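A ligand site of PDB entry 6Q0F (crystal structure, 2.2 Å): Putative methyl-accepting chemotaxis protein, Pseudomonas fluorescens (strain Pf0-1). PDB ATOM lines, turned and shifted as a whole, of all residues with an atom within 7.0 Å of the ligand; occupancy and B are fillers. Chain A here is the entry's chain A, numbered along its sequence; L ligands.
Residues that only touch the ligand: Ile 126 (3.3 Å), Phe 82 (3.4 Å), Phe 94 (3.5 Å), Met 90 (3.5 Å), Tyr 74 (3.6 Å), Ala 121 (3.7 Å) and Ile 84 (3.9 Å).
Hydrophobic or aromatic side chains that line the ligand: Tyr 74, Phe 82, Ile 84, Met 90, Phe 94, Trp 101, Tyr 117, Ala 120, Ala 121 and Ile 126.
13 residues have an atom within 4 Å of the ligand: Tyr 74, Phe 82, Ile 84, Met 90, Phe 94, Arg 99, Trp 101, Tyr 117, Asp 119, Ala 120, Ala 121, Ile 126 and Asp 146.
The nearest printed residue that does not touch the ligand is Ile 118 (4.3 Å).
OD2 of Asp 146 lies within salt-bridge range of N1 of the ligand (2.7 Å).
An oxygen (O1) of the ligand is in salt-bridge range of the guanidinium group (NE) of Arg 99 (2.7 Å).
NE1 of Trp 101 lies within hydrogen-bond range of O1 of the ligand, 2.8 Å away.
A nitrogen (N1) of the ligand is in salt-bridge range of the side-chain carboxylate of Asp 119 (2.8 Å).
The side-chain hydroxyl (OH) of Tyr 117 lies within hydrogen-bond range of a nitrogen (N1) of the ligand (2.9 Å).
N of Ala 120 is in hydrogen-bond range of O2 of the ligand (3.1 Å).
The side-chain hydroxyl of Tyr 74 is in hydrogen-bond range of the side-chain carboxylate of Asp 146 (2.6 Å).
OD1 of Asp 146 sits at hydrogen-bond distance from OG of Ser 128, 2.6 Å away.
N of Met 71 sits at hydrogen-bond distance from O of Asp 146.
The guanidinium group of Arg 99 sits at hydrogen-bond distance from the backbone carbonyl oxygen of Ile 118 (2.9 Å).
OD1 of Asp 119 lies within hydrogen-bond range of N of Ala 121, 3.2 Å away.
The backbone NH of Thr 122 lies within hydrogen-bond range of the side-chain carboxylate of Asp 119, 2.8 Å away.
O of Tyr 117 lies within hydrogen-bond range of N of Ile 126.
The side-chain hydroxyl (OH) of Tyr 117 lies within hydrogen-bond range of the side-chain hydroxyl (OG) of Ser 128 (2.4 Å).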
ATOM      1  N   MET A  71       6.401 -25.442 -13.099  1.00  0.00           N
ATOM      2  CA  MET A  71       5.394 -25.051 -14.111  1.00  0.00           C
ATOM      3  C   MET A  71       6.111 -24.310 -15.241  1.00  0.00           C
ATOM      4  O   MET A  71       5.807 -24.557 -16.415  1.00  0.00           O
ATOM      5  CB  MET A  71       4.326 -24.151 -13.504  1.00  0.00           C
ATOM      6  CG  MET A  71       3.515 -24.844 -12.443  1.00  0.00           C
ATOM      7  SD  MET A  71       2.493 -23.662 -11.507  1.00  0.00           S
ATOM      8  CE  MET A  71       3.690 -22.421 -11.048  1.00  0.00           C
ATOM      9  N   ALA A  72       7.087 -23.477 -14.896  1.00  0.00           N
ATOM     10  CA  ALA A  72       8.016 -22.849 -15.846  1.00  0.00           C
ATOM     11  C   ALA A  72       9.209 -22.332 -15.057  1.00  0.00           C
ATOM     12  O   ALA A  72       9.114 -22.257 -13.808  1.00  0.00           O
ATOM     13  CB  ALA A  72       7.367 -21.719 -16.629  1.00  0.00           C
ATOM     14  N   SER A  73      10.262 -21.962 -15.775  1.00  0.00           N
ATOM     15  CA  SER A  73      11.423 -21.263 -15.189  1.00  0.00           C
ATOM     16  C   SER A  73      11.858 -20.194 -16.180  1.00  0.00           C
ATOM     17  O   SER A  73      11.513 -20.288 -17.354  1.00  0.00           O
ATOM     18  CB  SER A  73      12.548 -22.230 -14.844  1.00  0.00           C
ATOM     19  OG  SER A  73      13.003 -22.948 -15.989  1.00  0.00           O
ATOM     20  N   TYR A  74      12.599 -19.192 -15.713  1.00  0.00           N
ATOM     21  CA  TYR A  74      12.684 -17.904 -16.434  1.00  0.00           C
ATOM     22  C   TYR A  74      13.910 -17.162 -15.915  1.00  0.00           C
ATOM     23  O   TYR A  74      14.514 -17.457 -14.836  1.00  0.00           O
ATOM     24  CB  TYR A  74      11.347 -17.157 -16.307  1.00  0.00           C
ATOM     25  CG  TYR A  74      10.762 -17.173 -14.920  1.00  0.00           C
ATOM     26  CD1 TYR A  74      11.263 -16.360 -13.918  1.00  0.00           C
ATOM     27  CD2 TYR A  74       9.818 -18.131 -14.568  1.00  0.00           C
ATOM     28  CE1 TYR A  74      10.797 -16.460 -12.617  1.00  0.00           C
ATOM     29  CE2 TYR A  74       9.333 -18.222 -13.273  1.00  0.00           C
ATOM     30  CZ  TYR A  74       9.803 -17.370 -12.294  1.00  0.00           C
ATOM     31  OH  TYR A  74       9.365 -17.512 -10.998  1.00  0.00           O
ATOM     32  N   LEU A  75      14.317 -16.208 -16.742  1.00  0.00           N
ATOM     33  CA  LEU A  75      15.353 -15.224 -16.376  1.00  0.00           C
ATOM     34  C   LEU A  75      14.783 -13.830 -16.631  1.00  0.00           C
ATOM     35  O   LEU A  75      14.304 -13.598 -17.758  1.00  0.00           O
ATOM     36  CB  LEU A  75      16.594 -15.432 -17.232  1.00  0.00           C
ATOM     37  CG  LEU A  75      17.649 -14.367 -16.992  1.00  0.00           C
ATOM     38  CD1 LEU A  75      18.370 -14.616 -15.684  1.00  0.00           C
ATOM     39  CD2 LEU A  75      18.636 -14.302 -18.148  1.00  0.00           C
ATOM     40  N   PHE A  82      13.543 -10.726 -20.630  1.00  0.00           N
ATOM     41  CA  PHE A  82      12.739 -11.806 -20.019  1.00  0.00           C
ATOM     42  C   PHE A  82      12.751 -13.003 -20.966  1.00  0.00           C
ATOM     43  O   PHE A  82      12.439 -12.851 -22.148  1.00  0.00           O
ATOM     44  CB  PHE A  82      11.316 -11.323 -19.771  1.00  0.00           C
ATOM     45  CG  PHE A  82      10.506 -12.392 -19.082  1.00  0.00           C
ATOM     46  CD1 PHE A  82      10.822 -12.781 -17.788  1.00  0.00           C
ATOM     47  CD2 PHE A  82       9.381 -12.923 -19.690  1.00  0.00           C
ATOM     48  CE1 PHE A  82      10.033 -13.696 -17.112  1.00  0.00           C
ATOM     49  CE2 PHE A  82       8.619 -13.855 -19.007  1.00  0.00           C
ATOM     50  CZ  PHE A  82       8.930 -14.221 -17.729  1.00  0.00           C
ATOM     51  N   THR A  83      13.088 -14.154 -20.411  1.00  0.00           N
ATOM     52  CA  THR A  83      13.005 -15.456 -21.088  1.00  0.00           C
ATOM     53  C   THR A  83      12.333 -16.417 -20.117  1.00  0.00           C
ATOM     54  O   THR A  83      12.834 -16.534 -18.983  1.00  0.00           O
ATOM     55  CB  THR A  83      14.402 -15.940 -21.477  1.00  0.00           C
ATOM     56  OG1 THR A  83      14.946 -14.887 -22.276  1.00  0.00           O
ATOM     57  CG2 THR A  83      14.368 -17.242 -22.251  1.00  0.00           C
ATOM     58  N   ILE A  84      11.297 -17.107 -20.600  1.00  0.00           N
ATOM     59  CA  ILE A  84      10.537 -18.142 -19.842  1.00  0.00           C
ATOM     60  C   ILE A  84      10.389 -19.401 -20.710  1.00  0.00           C
ATOM     61  O   ILE A  84      10.219 -19.284 -21.930  1.00  0.00           O
ATOM     62  CB  ILE A  84       9.171 -17.573 -19.393  1.00  0.00           C
ATOM     63  CG1 ILE A  84       8.368 -18.635 -18.635  1.00  0.00           C
ATOM     64  CG2 ILE A  84       8.415 -17.028 -20.587  1.00  0.00           C
ATOM     65  CD1 ILE A  84       7.307 -18.084 -17.718  1.00  0.00           C
ATOM     66  N   MET A  90       3.158 -12.978 -22.164  1.00  0.00           N
ATOM     67  CA  MET A  90       2.960 -12.319 -20.849  1.00  0.00           C
ATOM     68  C   MET A  90       1.981 -11.159 -21.028  1.00  0.00           C
ATOM     69  O   MET A  90       1.863 -10.569 -22.097  1.00  0.00           O
ATOM     70  CB  MET A  90       4.279 -11.881 -20.226  1.00  0.00           C
ATOM     71  CG  MET A  90       5.263 -13.034 -19.991  1.00  0.00           C
ATOM     72  SD  MET A  90       4.619 -14.430 -19.017  1.00  0.00           S
ATOM     73  CE  MET A  90       4.381 -13.609 -17.445  1.00  0.00           C
ATOM     74  N   PHE A  94       3.658  -6.378 -18.410  1.00  0.00           N
ATOM     75  CA  PHE A  94       4.442  -7.246 -17.497  1.00  0.00           C
ATOM     76  C   PHE A  94       5.880  -6.720 -17.516  1.00  0.00           C
ATOM     77  O   PHE A  94       6.422  -6.353 -18.553  1.00  0.00           O
ATOM     78  CB  PHE A  94       4.336  -8.697 -17.934  1.00  0.00           C
ATOM     79  CG  PHE A  94       5.308  -9.630 -17.259  1.00  0.00           C
ATOM     80  CD1 PHE A  94       5.039 -10.134 -15.994  1.00  0.00           C
ATOM     81  CD2 PHE A  94       6.513  -9.944 -17.850  1.00  0.00           C
ATOM     82  CE1 PHE A  94       5.926 -10.998 -15.383  1.00  0.00           C
ATOM     83  CE2 PHE A  94       7.386 -10.835 -17.248  1.00  0.00           C
ATOM     84  CZ  PHE A  94       7.081 -11.372 -16.020  1.00  0.00           C
ATOM     85  N   ASP A  95       6.470  -6.618 -16.336  1.00  0.00           N
ATOM     86  CA  ASP A  95       7.909  -6.288 -16.161  1.00  0.00           C
ATOM     87  C   ASP A  95       8.427  -7.259 -15.114  1.00  0.00           C
ATOM     88  O   ASP A  95       7.888  -7.296 -13.999  1.00  0.00           O
ATOM     89  CB  ASP A  95       8.038  -4.830 -15.720  1.00  0.00           C
ATOM     90  CG  ASP A  95       9.458  -4.404 -15.383  1.00  0.00           C
ATOM     91  OD1 ASP A  95      10.338  -5.303 -15.246  1.00  0.00           O
ATOM     92  OD2 ASP A  95       9.659  -3.176 -15.315  1.00  0.00           O
ATOM     93  N   PRO A  96       9.435  -8.096 -15.423  1.00  0.00           N
ATOM     94  CA  PRO A  96       9.960  -9.021 -14.423  1.00  0.00           C
ATOM     95  C   PRO A  96      10.446  -8.333 -13.128  1.00  0.00           C
ATOM     96  O   PRO A  96      10.436  -8.946 -12.081  1.00  0.00           O
ATOM     97  CB  PRO A  96      11.116  -9.735 -15.152  1.00  0.00           C
ATOM     98  CG  PRO A  96      11.472  -8.824 -16.305  1.00  0.00           C
ATOM     99  CD  PRO A  96      10.177  -8.135 -16.697  1.00  0.00           C
ATOM    100  N   ARG A  99       8.184  -7.998 -10.048  1.00  0.00           N
ATOM    101  CA  ARG A  99       7.567  -9.265  -9.597  1.00  0.00           C
ATOM    102  C   ARG A  99       8.194  -9.640  -8.268  1.00  0.00           C
ATOM    103  O   ARG A  99       9.294  -9.195  -7.956  1.00  0.00           O
ATOM    104  CB  ARG A  99       7.697 -10.318 -10.706  1.00  0.00           C
ATOM    105  CG  ARG A  99       7.053  -9.877 -12.013  1.00  0.00           C
ATOM    106  CD  ARG A  99       5.554  -9.603 -11.899  1.00  0.00           C
ATOM    107  NE  ARG A  99       4.762 -10.809 -11.782  1.00  0.00           N
ATOM    108  CZ  ARG A  99       3.547 -10.899 -11.246  1.00  0.00           C
ATOM    109  NH1 ARG A  99       2.917  -9.835 -10.795  1.00  0.00           N
ATOM    110  NH2 ARG A  99       2.915 -12.071 -11.233  1.00  0.00           N
ATOM    111  N   PRO A 100       7.462 -10.389  -7.415  1.00  0.00           N
ATOM    112  CA  PRO A 100       7.920 -10.769  -6.084  1.00  0.00           C
ATOM    113  C   PRO A 100       9.206 -11.614  -6.138  1.00  0.00           C
ATOM    114  O   PRO A 100       9.976 -11.546  -5.198  1.00  0.00           O
ATOM    115  CB  PRO A 100       6.807 -11.686  -5.558  1.00  0.00           C
ATOM    116  CG  PRO A 100       5.584 -11.311  -6.364  1.00  0.00           C
ATOM    117  CD  PRO A 100       6.136 -10.958  -7.729  1.00  0.00           C
ATOM    118  N   TRP A 101       9.305 -12.530  -7.109  1.00  0.00           N
ATOM    119  CA  TRP A 101      10.447 -13.468  -7.205  1.00  0.00           C
ATOM    120  C   TRP A 101      11.703 -12.641  -7.455  1.00  0.00           C
ATOM    121  O   TRP A 101      12.751 -12.995  -6.914  1.00  0.00           O
ATOM    122  CB  TRP A 101      10.229 -14.526  -8.290  1.00  0.00           C
ATOM    123  CG  TRP A 101       9.834 -13.995  -9.635  1.00  0.00           C
ATOM    124  CD1 TRP A 101       8.558 -13.888 -10.115  1.00  0.00           C
ATOM    125  CD2 TRP A 101      10.705 -13.558 -10.687  1.00  0.00           C
ATOM    126  NE1 TRP A 101       8.596 -13.420 -11.405  1.00  0.00           N
ATOM    127  CE2 TRP A 101       9.885 -13.231 -11.788  1.00  0.00           C
ATOM    128  CE3 TRP A 101      12.086 -13.604 -10.895  1.00  0.00           C
ATOM    129  CZ2 TRP A 101      10.402 -12.879 -13.036  1.00  0.00           C
ATOM    130  CZ3 TRP A 101      12.593 -13.235 -12.115  1.00  0.00           C
ATOM    131  CH2 TRP A 101      11.772 -12.866 -13.170  1.00  0.00           C
ATOM    132  N   TYR A 117       1.586 -15.914  -4.459  1.00  0.00           N
ATOM    133  CA  TYR A 117       1.142 -14.746  -5.242  1.00  0.00           C
ATOM    134  C   TYR A 117       0.381 -15.276  -6.467  1.00  0.00           C
ATOM    135  O   TYR A 117       0.255 -16.519  -6.626  1.00  0.00           O
ATOM    136  CB  TYR A 117       2.364 -13.885  -5.557  1.00  0.00           C
ATOM    137  CG  TYR A 117       3.331 -14.496  -6.545  1.00  0.00           C
ATOM    138  CD1 TYR A 117       4.369 -15.324  -6.144  1.00  0.00           C
ATOM    139  CD2 TYR A 117       3.323 -14.126  -7.885  1.00  0.00           C
ATOM    140  CE1 TYR A 117       5.300 -15.843  -7.031  1.00  0.00           C
ATOM    141  CE2 TYR A 117       4.250 -14.622  -8.789  1.00  0.00           C
ATOM    142  CZ  TYR A 117       5.246 -15.488  -8.379  1.00  0.00           C
ATOM    143  OH  TYR A 117       6.129 -15.984  -9.308  1.00  0.00           O
ATOM    144  N   ILE A 118      -0.041 -14.362  -7.338  1.00  0.00           N
ATOM    145  CA  ILE A 118      -0.830 -14.659  -8.565  1.00  0.00           C
ATOM    146  C   ILE A 118       0.105 -14.697  -9.777  1.00  0.00           C
ATOM    147  O   ILE A 118       0.709 -13.684 -10.135  1.00  0.00           O
ATOM    148  CB  ILE A 118      -2.008 -13.653  -8.696  1.00  0.00           C
ATOM    149  CG1 ILE A 118      -2.879 -13.717  -7.435  1.00  0.00           C
ATOM    150  CG2 ILE A 118      -2.816 -13.916  -9.967  1.00  0.00           C
ATOM    151  CD1 ILE A 118      -3.542 -12.429  -7.055  1.00  0.00           C
ATOM    152  N   ASP A 119       0.255 -15.879 -10.374  1.00  0.00           N
ATOM    153  CA  ASP A 119       1.062 -16.075 -11.600  1.00  0.00           C
ATOM    154  C   ASP A 119       0.565 -15.100 -12.672  1.00  0.00           C
ATOM    155  O   ASP A 119      -0.642 -15.141 -12.984  1.00  0.00           O
ATOM    156  CB  ASP A 119       0.966 -17.531 -12.059  1.00  0.00           C
ATOM    157  CG  ASP A 119       1.972 -17.906 -13.133  1.00  0.00           C
ATOM    158  OD1 ASP A 119       3.000 -17.216 -13.256  1.00  0.00           O
ATOM    159  OD2 ASP A 119       1.680 -18.833 -13.884  1.00  0.00           O
ATOM    160  N   ALA A 120       1.477 -14.313 -13.252  1.00  0.00           N
ATOM    161  CA  ALA A 120       1.277 -13.505 -14.474  1.00  0.00           C
ATOM    162  C   ALA A 120       0.998 -14.420 -15.662  1.00  0.00           C
ATOM    163  O   ALA A 120       0.276 -13.970 -16.570  1.00  0.00           O
ATOM    164  CB  ALA A 120       2.491 -12.662 -14.715  1.00  0.00           C
ATOM    165  N   ALA A 121       1.621 -15.612 -15.691  1.00  0.00           N
ATOM    166  CA  ALA A 121       1.579 -16.593 -16.801  1.00  0.00           C
ATOM    167  C   ALA A 121       0.218 -17.308 -16.832  1.00  0.00           C
ATOM    168  O   ALA A 121      -0.409 -17.318 -17.912  1.00  0.00           O
ATOM    169  CB  ALA A 121       2.706 -17.593 -16.709  1.00  0.00           C
ATOM    170  N   THR A 122      -0.155 -17.992 -15.753  1.00  0.00           N
ATOM    171  CA  THR A 122      -1.359 -18.872 -15.687  1.00  0.00           C
ATOM    172  C   THR A 122      -2.511 -18.168 -14.986  1.00  0.00           C
ATOM    173  O   THR A 122      -3.632 -18.654 -15.142  1.00  0.00           O
ATOM    174  CB  THR A 122      -1.089 -20.187 -14.950  1.00  0.00           C
ATOM    175  OG1 THR A 122      -0.858 -19.852 -13.587  1.00  0.00           O
ATOM    176  CG2 THR A 122       0.094 -20.940 -15.520  1.00  0.00           C
ATOM    177  N   ILE A 126       0.643 -19.450  -6.856  1.00  0.00           N
ATOM    178  CA  ILE A 126       1.951 -20.156  -6.992  1.00  0.00           C
ATOM    179  C   ILE A 126       2.886 -19.635  -5.909  1.00  0.00           C
ATOM    180  O   ILE A 126       2.632 -18.550  -5.358  1.00  0.00           O
ATOM    181  CB  ILE A 126       2.537 -19.923  -8.397  1.00  0.00           C
ATOM    182  CG1 ILE A 126       2.953 -18.452  -8.574  1.00  0.00           C
ATOM    183  CG2 ILE A 126       1.574 -20.388  -9.468  1.00  0.00           C
ATOM    184  CD1 ILE A 126       3.854 -18.209  -9.743  1.00  0.00           C
ATOM    185  N   ILE A 127       3.996 -20.348  -5.698  1.00  0.00           N
ATOM    186  CA  ILE A 127       5.198 -19.773  -5.038  1.00  0.00           C
ATOM    187  C   ILE A 127       6.347 -19.907  -6.037  1.00  0.00           C
ATOM    188  O   ILE A 127       6.290 -20.798  -6.897  1.00  0.00           O
ATOM    189  CB  ILE A 127       5.511 -20.433  -3.678  1.00  0.00           C
ATOM    190  CG1 ILE A 127       6.057 -21.850  -3.862  1.00  0.00           C
ATOM    191  CG2 ILE A 127       4.310 -20.376  -2.759  1.00  0.00           C
ATOM    192  CD1 ILE A 127       6.855 -22.343  -2.655  1.00  0.00           C
ATOM    193  N   SER A 128       7.360 -19.073  -5.896  1.00  0.00           N
ATOM    194  CA  SER A 128       8.567 -19.122  -6.745  1.00  0.00           C
ATOM    195  C   SER A 128       9.805 -19.360  -5.862  1.00  0.00           C
ATOM    196  O   SER A 128       9.814 -18.828  -4.729  1.00  0.00           O
ATOM    197  CB  SER A 128       8.643 -17.860  -7.584  1.00  0.00           C
ATOM    198  OG  SER A 128       7.543 -17.755  -8.478  1.00  0.00           O
ATOM    199  N   GLY A 145      11.747 -20.367 -10.710  1.00  0.00           N
ATOM    200  CA  GLY A 145      10.964 -21.578 -10.980  1.00  0.00           C
ATOM    201  C   GLY A 145       9.666 -21.546 -10.192  1.00  0.00           C
ATOM    202  O   GLY A 145       9.735 -21.175  -9.004  1.00  0.00           O
ATOM    203  N   ASP A 146       8.544 -21.885 -10.829  1.00  0.00           N
ATOM    204  CA  ASP A 146       7.175 -21.735 -10.262  1.00  0.00           C
ATOM    205  C   ASP A 146       6.696 -23.106  -9.834  1.00  0.00           C
ATOM    206  O   ASP A 146       6.875 -24.078 -10.598  1.00  0.00           O
ATOM    207  CB  ASP A 146       6.192 -21.065 -11.237  1.00  0.00           C
ATOM    208  CG  ASP A 146       6.560 -19.627 -11.520  1.00  0.00           C
ATOM    209  OD1 ASP A 146       7.256 -19.020 -10.684  1.00  0.00           O
ATOM    210  OD2 ASP A 146       6.173 -19.134 -12.591  1.00  0.00           O
HETATM  211  N1  LIG L   1       5.492 -16.598 -12.084  1.00  0.00           N
HETATM  212  C1  LIG L   1       6.347 -15.511 -12.650  1.00  0.00           C
HETATM  213  C2  LIG L   1       5.586 -14.183 -12.495  1.00  0.00           C
HETATM  214  O1  LIG L   1       6.086 -13.053 -12.592  1.00  0.00           O
HETATM  215  C3  LIG L   1       6.760 -15.830 -14.100  1.00  0.00           C
HETATM  216  C4  LIG L   1       5.563 -15.854 -15.050  1.00  0.00           C
HETATM  217  C5  LIG L   1       7.809 -14.861 -14.612  1.00  0.00           C
HETATM  218  O2  LIG L   1       4.395 -14.259 -12.226  1.00  0.00           O
